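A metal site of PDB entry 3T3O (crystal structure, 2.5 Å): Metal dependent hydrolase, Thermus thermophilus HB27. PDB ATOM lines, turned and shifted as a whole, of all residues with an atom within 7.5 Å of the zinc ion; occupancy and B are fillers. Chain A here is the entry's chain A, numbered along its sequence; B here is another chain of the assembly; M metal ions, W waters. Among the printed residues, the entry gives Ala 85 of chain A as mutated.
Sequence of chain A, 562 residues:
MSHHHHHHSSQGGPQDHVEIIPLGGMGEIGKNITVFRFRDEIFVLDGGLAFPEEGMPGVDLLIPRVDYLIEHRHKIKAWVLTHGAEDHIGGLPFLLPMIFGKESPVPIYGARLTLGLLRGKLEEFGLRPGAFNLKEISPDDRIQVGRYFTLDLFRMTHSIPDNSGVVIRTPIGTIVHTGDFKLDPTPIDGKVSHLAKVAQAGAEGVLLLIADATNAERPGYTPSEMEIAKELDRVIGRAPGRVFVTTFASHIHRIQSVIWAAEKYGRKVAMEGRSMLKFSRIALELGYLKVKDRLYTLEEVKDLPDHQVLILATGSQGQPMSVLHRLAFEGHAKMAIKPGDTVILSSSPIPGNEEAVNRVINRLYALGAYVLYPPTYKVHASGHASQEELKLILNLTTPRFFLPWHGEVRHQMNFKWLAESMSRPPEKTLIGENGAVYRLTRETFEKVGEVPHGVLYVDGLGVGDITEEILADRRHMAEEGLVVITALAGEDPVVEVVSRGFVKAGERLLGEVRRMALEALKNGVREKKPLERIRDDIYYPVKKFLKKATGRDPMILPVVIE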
ATOM      1  N   ILE A  29      33.643  -8.342   5.783  1.00  0.00           N
ATOM      2  CA  ILE A  29      32.418  -8.474   5.000  1.00  0.00           C
ATOM      3  C   ILE A  29      31.898  -9.940   4.810  1.00  0.00           C
ATOM      4  O   ILE A  29      30.678 -10.160   4.817  1.00  0.00           O
ATOM      5  CB  ILE A  29      32.455  -7.560   3.727  1.00  0.00           C
ATOM      6  CG1 ILE A  29      32.189  -6.088   4.095  1.00  0.00           C
ATOM      7  CG2 ILE A  29      31.496  -7.993   2.632  1.00  0.00           C
ATOM      8  CD1 ILE A  29      33.411  -5.223   4.231  1.00  0.00           C
ATOM      9  N   GLY A  30      32.823 -10.915   4.709  1.00  0.00           N
ATOM     10  CA  GLY A  30      32.501 -12.332   4.521  1.00  0.00           C
ATOM     11  C   GLY A  30      32.524 -13.219   5.760  1.00  0.00           C
ATOM     12  O   GLY A  30      32.646 -12.714   6.881  1.00  0.00           O
ATOM     13  N   LYS A  31      32.428 -14.550   5.534  1.00  0.00           N
ATOM     14  CA  LYS A  31      32.395 -15.642   6.524  1.00  0.00           C
ATOM     15  C   LYS A  31      31.552 -15.387   7.785  1.00  0.00           C
ATOM     16  O   LYS A  31      31.987 -15.606   8.914  1.00  0.00           O
ATOM     17  CB  LYS A  31      33.766 -16.296   6.810  1.00  0.00           C
ATOM     18  CG  LYS A  31      34.784 -15.390   7.485  1.00  0.00           C
ATOM     19  CD  LYS A  31      36.134 -16.091   7.632  1.00  0.00           C
ATOM     20  CE  LYS A  31      37.230 -15.124   8.018  1.00  0.00           C
ATOM     21  NZ  LYS A  31      37.030 -14.536   9.382  1.00  0.00           N
ATOM     22  N   ASN A  32      30.323 -14.922   7.573  1.00  0.00           N
ATOM     23  CA  ASN A  32      29.369 -14.615   8.631  1.00  0.00           C
ATOM     24  C   ASN A  32      28.915 -15.876   9.364  1.00  0.00           C
ATOM     25  O   ASN A  32      28.558 -16.877   8.750  1.00  0.00           O
ATOM     26  CB  ASN A  32      28.172 -13.872   8.056  1.00  0.00           C
ATOM     27  CG  ASN A  32      28.530 -12.495   7.549  1.00  0.00           C
ATOM     28  OD1 ASN A  32      28.490 -11.511   8.288  1.00  0.00           O
ATOM     29  ND2 ASN A  32      28.921 -12.422   6.292  1.00  0.00           N
ATOM     30  N   THR A  82      19.951 -17.072   7.123  1.00  0.00           N
ATOM     31  CA  THR A  82      19.293 -15.867   6.597  1.00  0.00           C
ATOM     32  C   THR A  82      19.159 -15.796   5.073  1.00  0.00           C
ATOM     33  O   THR A  82      18.185 -15.224   4.599  1.00  0.00           O
ATOM     34  CB  THR A  82      19.874 -14.569   7.214  1.00  0.00           C
ATOM     35  OG1 THR A  82      21.184 -14.299   6.698  1.00  0.00           O
ATOM     36  CG2 THR A  82      19.881 -14.582   8.747  1.00  0.00           C
ATOM     37  N   HIS A  83      20.141 -16.331   4.302  1.00  0.00           N
ATOM     38  CA  HIS A  83      20.169 -16.387   2.826  1.00  0.00           C
ATOM     39  C   HIS A  83      21.167 -17.374   2.228  1.00  0.00           C
ATOM     40  O   HIS A  83      22.081 -17.806   2.934  1.00  0.00           O
ATOM     41  CB  HIS A  83      20.244 -15.006   2.139  1.00  0.00           C
ATOM     42  CG  HIS A  83      21.424 -14.160   2.504  1.00  0.00           C
ATOM     43  ND1 HIS A  83      21.583 -13.661   3.781  1.00  0.00           N
ATOM     44  CD2 HIS A  83      22.390 -13.643   1.710  1.00  0.00           C
ATOM     45  CE1 HIS A  83      22.662 -12.891   3.738  1.00  0.00           C
ATOM     46  NE2 HIS A  83      23.181 -12.853   2.509  1.00  0.00           N
ATOM     47  N   ALA A  85      23.511 -16.991  -0.104  1.00  0.00           N
ATOM     48  CA  ALA A  85      24.777 -16.482  -0.659  1.00  0.00           C
ATOM     49  C   ALA A  85      25.956 -17.165   0.027  1.00  0.00           C
ATOM     50  O   ALA A  85      25.878 -17.490   1.229  1.00  0.00           O
ATOM     51  CB  ALA A  85      24.860 -14.968  -0.487  1.00  0.00           C
ATOM     52  N   GLU A  86      27.055 -17.383  -0.730  1.00  0.00           N
ATOM     53  CA  GLU A  86      28.314 -18.028  -0.304  1.00  0.00           C
ATOM     54  C   GLU A  86      28.843 -17.539   1.024  1.00  0.00           C
ATOM     55  O   GLU A  86      29.331 -18.351   1.805  1.00  0.00           O
ATOM     56  CB  GLU A  86      29.403 -17.887  -1.382  1.00  0.00           C
ATOM     57  CG  GLU A  86      29.122 -18.620  -2.675  1.00  0.00           C
ATOM     58  CD  GLU A  86      29.258 -20.136  -2.677  1.00  0.00           C
ATOM     59  OE1 GLU A  86      28.925 -20.747  -3.715  1.00  0.00           O
ATOM     60  OE2 GLU A  86      29.669 -20.706  -1.647  1.00  0.00           O
ATOM     61  N   ASP A  87      28.734 -16.221   1.319  1.00  0.00           N
ATOM     62  CA  ASP A  87      29.224 -15.668   2.582  1.00  0.00           C
ATOM     63  C   ASP A  87      28.274 -15.875   3.783  1.00  0.00           C
ATOM     64  O   ASP A  87      28.486 -15.312   4.860  1.00  0.00           O
ATOM     65  CB  ASP A  87      29.691 -14.203   2.421  1.00  0.00           C
ATOM     66  CG  ASP A  87      28.570 -13.190   2.419  1.00  0.00           C
ATOM     67  OD1 ASP A  87      27.667 -13.288   1.550  1.00  0.00           O
ATOM     68  OD2 ASP A  87      28.600 -12.297   3.292  1.00  0.00           O
ATOM     69  N   HIS A  88      27.218 -16.680   3.566  1.00  0.00           N
ATOM     70  CA  HIS A  88      26.249 -17.041   4.594  1.00  0.00           C
ATOM     71  C   HIS A  88      26.013 -18.554   4.677  1.00  0.00           C
ATOM     72  O   HIS A  88      25.744 -19.056   5.766  1.00  0.00           O
ATOM     73  CB  HIS A  88      24.956 -16.213   4.489  1.00  0.00           C
ATOM     74  CG  HIS A  88      25.144 -14.809   4.986  1.00  0.00           C
ATOM     75  ND1 HIS A  88      24.798 -14.446   6.287  1.00  0.00           N
ATOM     76  CD2 HIS A  88      25.722 -13.746   4.382  1.00  0.00           C
ATOM     77  CE1 HIS A  88      25.156 -13.179   6.405  1.00  0.00           C
ATOM     78  NE2 HIS A  88      25.710 -12.715   5.297  1.00  0.00           N
ATOM     79  N   HIS A 158      17.543  -7.832  -0.781  1.00  0.00           N
ATOM     80  CA  HIS A 158      18.998  -7.928  -0.918  1.00  0.00           C
ATOM     81  C   HIS A 158      19.379  -8.341  -2.371  1.00  0.00           C
ATOM     82  O   HIS A 158      18.640  -7.966  -3.292  1.00  0.00           O
ATOM     83  CB  HIS A 158      19.562  -8.869   0.176  1.00  0.00           C
ATOM     84  CG  HIS A 158      21.053  -8.943   0.280  1.00  0.00           C
ATOM     85  ND1 HIS A 158      21.840  -7.803   0.344  1.00  0.00           N
ATOM     86  CD2 HIS A 158      21.864 -10.037   0.356  1.00  0.00           C
ATOM     87  CE1 HIS A 158      23.094  -8.235   0.430  1.00  0.00           C
ATOM     88  NE2 HIS A 158      23.158  -9.572   0.458  1.00  0.00           N
ATOM     89  N   SER A 159      20.513  -9.040  -2.579  1.00  0.00           N
ATOM     90  CA  SER A 159      21.019  -9.431  -3.912  1.00  0.00           C
ATOM     91  C   SER A 159      20.477 -10.775  -4.358  1.00  0.00           C
ATOM     92  O   SER A 159      20.344 -11.040  -5.549  1.00  0.00           O
ATOM     93  CB  SER A 159      22.549  -9.427  -3.933  1.00  0.00           C
ATOM     94  OG  SER A 159      23.152  -9.367  -2.645  1.00  0.00           O
ATOM     95  N   ASN A 163      15.793 -13.716   1.252  1.00  0.00           N
ATOM     96  CA  ASN A 163      16.724 -13.215   2.234  1.00  0.00           C
ATOM     97  C   ASN A 163      15.978 -12.681   3.493  1.00  0.00           C
ATOM     98  O   ASN A 163      15.011 -11.920   3.382  1.00  0.00           O
ATOM     99  CB  ASN A 163      17.593 -12.144   1.589  1.00  0.00           C
ATOM    100  CG  ASN A 163      18.324 -11.283   2.564  1.00  0.00           C
ATOM    101  OD1 ASN A 163      17.932 -10.166   2.846  1.00  0.00           O
ATOM    102  ND2 ASN A 163      19.348 -11.810   3.152  1.00  0.00           N
ATOM    103  N   GLY A 179      19.954  -8.594   9.200  1.00  0.00           N
ATOM    104  CA  GLY A 179      20.515  -9.460   8.168  1.00  0.00           C
ATOM    105  C   GLY A 179      21.126  -8.596   7.071  1.00  0.00           C
ATOM    106  O   GLY A 179      21.213  -7.374   7.233  1.00  0.00           O
ATOM    107  N   ASP A 180      21.533  -9.202   5.947  1.00  0.00           N
ATOM    108  CA  ASP A 180      22.050  -8.430   4.815  1.00  0.00           C
ATOM    109  C   ASP A 180      20.829  -7.817   4.145  1.00  0.00           C
ATOM    110  O   ASP A 180      19.891  -8.545   3.830  1.00  0.00           O
ATOM    111  CB  ASP A 180      22.803  -9.305   3.827  1.00  0.00           C
ATOM    112  CG  ASP A 180      24.114  -9.847   4.352  1.00  0.00           C
ATOM    113  OD1 ASP A 180      24.103 -10.442   5.446  1.00  0.00           O
ATOM    114  OD2 ASP A 180      25.123  -9.756   3.635  1.00  0.00           O
ATOM    115  N   PHE A 181      20.788  -6.488   4.020  1.00  0.00           N
ATOM    116  CA  PHE A 181      19.604  -5.829   3.470  1.00  0.00           C
ATOM    117  C   PHE A 181      19.886  -4.510   2.766  1.00  0.00           C
ATOM    118  O   PHE A 181      20.941  -3.925   2.901  1.00  0.00           O
ATOM    119  CB  PHE A 181      18.547  -5.590   4.598  1.00  0.00           C
ATOM    120  CG  PHE A 181      18.733  -4.322   5.412  1.00  0.00           C
ATOM    121  CD1 PHE A 181      19.669  -4.264   6.436  1.00  0.00           C
ATOM    122  CD2 PHE A 181      17.992  -3.177   5.124  1.00  0.00           C
ATOM    123  CE1 PHE A 181      19.838  -3.087   7.177  1.00  0.00           C
ATOM    124  CE2 PHE A 181      18.188  -2.003   5.854  1.00  0.00           C
ATOM    125  CZ  PHE A 181      19.104  -1.966   6.876  1.00  0.00           C
ATOM    126  N   ASP A 212      23.613  -4.470   9.420  1.00  0.00           N
ATOM    127  CA  ASP A 212      24.427  -4.454   8.208  1.00  0.00           C
ATOM    128  C   ASP A 212      25.079  -3.072   8.040  1.00  0.00           C
ATOM    129  O   ASP A 212      24.390  -2.086   7.784  1.00  0.00           O
ATOM    130  CB  ASP A 212      23.473  -4.747   7.040  1.00  0.00           C
ATOM    131  CG  ASP A 212      24.106  -5.003   5.711  1.00  0.00           C
ATOM    132  OD1 ASP A 212      25.339  -4.901   5.621  1.00  0.00           O
ATOM    133  OD2 ASP A 212      23.373  -5.305   4.756  1.00  0.00           O
ATOM    134  N   THR A 214      27.773  -2.423   5.866  1.00  0.00           N
ATOM    135  CA  THR A 214      28.458  -2.354   4.562  1.00  0.00           C
ATOM    136  C   THR A 214      28.561  -0.954   3.979  1.00  0.00           C
ATOM    137  O   THR A 214      29.667  -0.565   3.623  1.00  0.00           O
ATOM    138  CB  THR A 214      27.837  -3.312   3.548  1.00  0.00           C
ATOM    139  OG1 THR A 214      27.489  -4.539   4.168  1.00  0.00           O
ATOM    140  CG2 THR A 214      28.736  -3.558   2.331  1.00  0.00           C
ATOM    141  N   HIS A 384      23.372  -3.658  -0.347  1.00  0.00           N
ATOM    142  CA  HIS A 384      23.351  -3.118   1.002  1.00  0.00           C
ATOM    143  C   HIS A 384      22.828  -1.685   1.117  1.00  0.00           C
ATOM    144  O   HIS A 384      23.126  -0.827   0.279  1.00  0.00           O
ATOM    145  CB  HIS A 384      24.710  -3.277   1.659  1.00  0.00           C
ATOM    146  CG  HIS A 384      25.227  -4.687   1.637  1.00  0.00           C
ATOM    147  ND1 HIS A 384      24.932  -5.581   2.655  1.00  0.00           N
ATOM    148  CD2 HIS A 384      26.015  -5.305   0.729  1.00  0.00           C
ATOM    149  CE1 HIS A 384      25.532  -6.708   2.319  1.00  0.00           C
ATOM    150  NE2 HIS A 384      26.185  -6.601   1.174  1.00  0.00           N
ATOM    151  N   TRP A 405      27.555  -4.651  12.310  1.00  0.00           N
ATOM    152  CA  TRP A 405      28.034  -5.923  11.793  1.00  0.00           C
ATOM    153  C   TRP A 405      28.137  -5.850  10.269  1.00  0.00           C
ATOM    154  O   TRP A 405      27.765  -4.834   9.697  1.00  0.00           O
ATOM    155  CB  TRP A 405      27.065  -7.020  12.308  1.00  0.00           C
ATOM    156  CG  TRP A 405      26.952  -8.257  11.477  1.00  0.00           C
ATOM    157  CD1 TRP A 405      27.799  -9.327  11.480  1.00  0.00           C
ATOM    158  CD2 TRP A 405      25.956  -8.534  10.489  1.00  0.00           C
ATOM    159  NE1 TRP A 405      27.399 -10.256  10.535  1.00  0.00           N
ATOM    160  CE2 TRP A 405      26.266  -9.790   9.924  1.00  0.00           C
ATOM    161  CE3 TRP A 405      24.840  -7.821  10.013  1.00  0.00           C
ATOM    162  CZ2 TRP A 405      25.486 -10.358   8.902  1.00  0.00           C
ATOM    163  CZ3 TRP A 405      24.077  -8.386   8.993  1.00  0.00           C
ATOM    164  CH2 TRP A 405      24.405  -9.632   8.452  1.00  0.00           C
ATOM    165  N   HIS A 406      28.688  -6.893   9.624  1.00  0.00           N
ATOM    166  CA  HIS A 406      28.864  -7.022   8.179  1.00  0.00           C
ATOM    167  C   HIS A 406      29.677  -5.880   7.524  1.00  0.00           C
ATOM    168  O   HIS A 406      29.398  -5.467   6.395  1.00  0.00           O
ATOM    169  CB  HIS A 406      27.528  -7.273   7.467  1.00  0.00           C
ATOM    170  CG  HIS A 406      27.681  -8.041   6.199  1.00  0.00           C
ATOM    171  ND1 HIS A 406      27.915  -7.406   4.996  1.00  0.00           N
ATOM    172  CD2 HIS A 406      27.644  -9.381   5.989  1.00  0.00           C
ATOM    173  CE1 HIS A 406      28.006  -8.366   4.085  1.00  0.00           C
ATOM    174  NE2 HIS A 406      27.842  -9.572   4.641  1.00  0.00           N
ATOM    175  N1  OMC B   1      31.692  -7.229  -0.926  1.00  0.00           N
ATOM    176  C2  OMC B   1      32.965  -7.016  -0.302  1.00  0.00           C
ATOM    177  N3  OMC B   1      33.355  -5.760   0.057  1.00  0.00           N
ATOM    178  C4  OMC B   1      32.565  -4.714  -0.165  1.00  0.00           C
ATOM    179  C5  OMC B   1      31.280  -4.850  -0.785  1.00  0.00           C
ATOM    180  C6  OMC B   1      30.891  -6.106  -1.144  1.00  0.00           C
ATOM    181  O2  OMC B   1      33.725  -7.930  -0.064  1.00  0.00           O
ATOM    182  N4  OMC B   1      33.016  -3.537   0.218  1.00  0.00           N
ATOM    183  C1' OMC B   1      31.181  -8.614  -1.373  1.00  0.00           C
ATOM    184  C2' OMC B   1      29.935  -9.271  -0.778  1.00  0.00           C
ATOM    185  O2' OMC B   1      30.277 -10.043   0.359  1.00  0.00           O
ATOM    186  CM2 OMC B   1      28.936  -9.896   1.087  1.00  0.00           C
ATOM    187  C3' OMC B   1      29.407 -10.112  -1.943  1.00  0.00           C
ATOM    188  C4' OMC B   1      29.844  -9.340  -3.181  1.00  0.00           C
ATOM    189  O4' OMC B   1      30.948  -8.508  -2.770  1.00  0.00           O
ATOM    190  O3' OMC B   1      29.950 -11.437  -1.984  1.00  0.00           O
ATOM    191  C5' OMC B   1      28.763  -8.507  -3.861  1.00  0.00           C
ATOM    192  O5' OMC B   1      28.279  -7.487  -2.998  1.00  0.00           O
ATOM    193  P   OMC B   1      27.114  -6.464  -3.428  1.00  0.00           P
ATOM    194  OP1 OMC B   1      26.785  -6.700  -4.857  1.00  0.00           O
ATOM    195  OP2 OMC B   1      26.042  -6.601  -2.426  1.00  0.00           O
ATOM    196  OP3 OMC B   1      27.494  -5.123  -3.437  1.00  0.00           O
ATOM    197  N1  OMU B   2      34.837 -11.881  -4.304  1.00  0.00           N
ATOM    198  C2  OMU B   2      36.100 -11.392  -4.544  1.00  0.00           C
ATOM    199  N3  OMU B   2      36.742 -10.799  -3.472  1.00  0.00           N
ATOM    200  C4  OMU B   2      36.249 -10.655  -2.198  1.00  0.00           C
ATOM    201  C5  OMU B   2      34.926 -11.188  -2.017  1.00  0.00           C
ATOM    202  C6  OMU B   2      34.287 -11.770  -3.046  1.00  0.00           C
ATOM    203  O2  OMU B   2      36.630 -11.478  -5.627  1.00  0.00           O
ATOM    204  O4  OMU B   2      36.911 -10.122  -1.330  1.00  0.00           O
ATOM    205  C1' OMU B   2      34.112 -12.521  -5.396  1.00  0.00           C
ATOM    206  C2' OMU B   2      34.223 -14.026  -5.602  1.00  0.00           C
ATOM    207  O2' OMU B   2      35.365 -14.308  -6.401  1.00  0.00           O
ATOM    208  CM2 OMU B   2      36.226 -15.541  -5.915  1.00  0.00           C
ATOM    209  C3' OMU B   2      32.893 -14.383  -6.283  1.00  0.00           C
ATOM    210  C4' OMU B   2      31.930 -13.307  -5.803  1.00  0.00           C
ATOM    211  O3' OMU B   2      32.991 -14.356  -7.707  1.00  0.00           O
ATOM    212  O4' OMU B   2      32.740 -12.179  -5.363  1.00  0.00           O
ATOM    213  C5' OMU B   2      30.981 -13.718  -4.685  1.00  0.00           C
ATOM    214  O5' OMU B   2      30.297 -12.563  -4.184  1.00  0.00           O
ATOM    215  P   OMU B   2      29.340 -12.601  -2.901  1.00  0.00           P
ATOM    216  OP1 OMU B   2      27.984 -12.193  -3.339  1.00  0.00           O
ATOM    217  OP2 OMU B   2      29.534 -13.885  -2.202  1.00  0.00           O
HETATM  218 ZN    ZN M   1      26.347 -11.142   3.242  1.00  0.00          ZN
HETATM  219  O   HOH W   1      25.438 -11.312   0.362  1.00  0.00           O
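The zinc ion is bound by OD2 of Asp 180 (1.9 Å), OD2 of Asp 87 (2.5 Å), NE2 of His 406 (2.6 Å) and NE2 of His 88 (2.7 Å).
ND2 of Asn 163 lies within hydrogen-bond range of ND1 of His 83 (3.0 Å). ND1 of His 406 is in hydrogen-bond range of OG1 of Thr 214. The backbone carbonyl oxygen of Ile 29 lies close to a ring nitrogen (NE2) of His 406, 2.9 Å away. NE2 of His 88 sits close to ND2 of Asn 32 (3.4 Å). The side-chain hydroxyl (OG1) of Thr 82 is in hydrogen-bond range of a ring nitrogen (ND1) of His 83, 3.0 Å away. O of Asp 180 sits close to OD1 of Asn 163, 2.7 Å away. A ring nitrogen (NE2) of His 406 lies close to the side-chain amide nitrogen of Asn 32, 3.5 Å away. The backbone carbonyl oxygen (O) of Asp 87 is in hydrogen-bond range of the side-chain amide nitrogen (ND2) of Asn 32 (3.3 Å).
Water W1 lies within hydrogen-bond range of a ring nitrogen (NE2) of His 158, the side-chain carboxylate of Asp 87 and a ring nitrogen (NE2) of His 83.
Residues that only touch the zinc ion: OMC 1 of chain B (3.6 Å) and His 83 (3.7 Å). Within 4 Å of the zinc ion: His 83, Asp 87, His 88, Asp 180, His 406 and OMC 1 of chain B.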
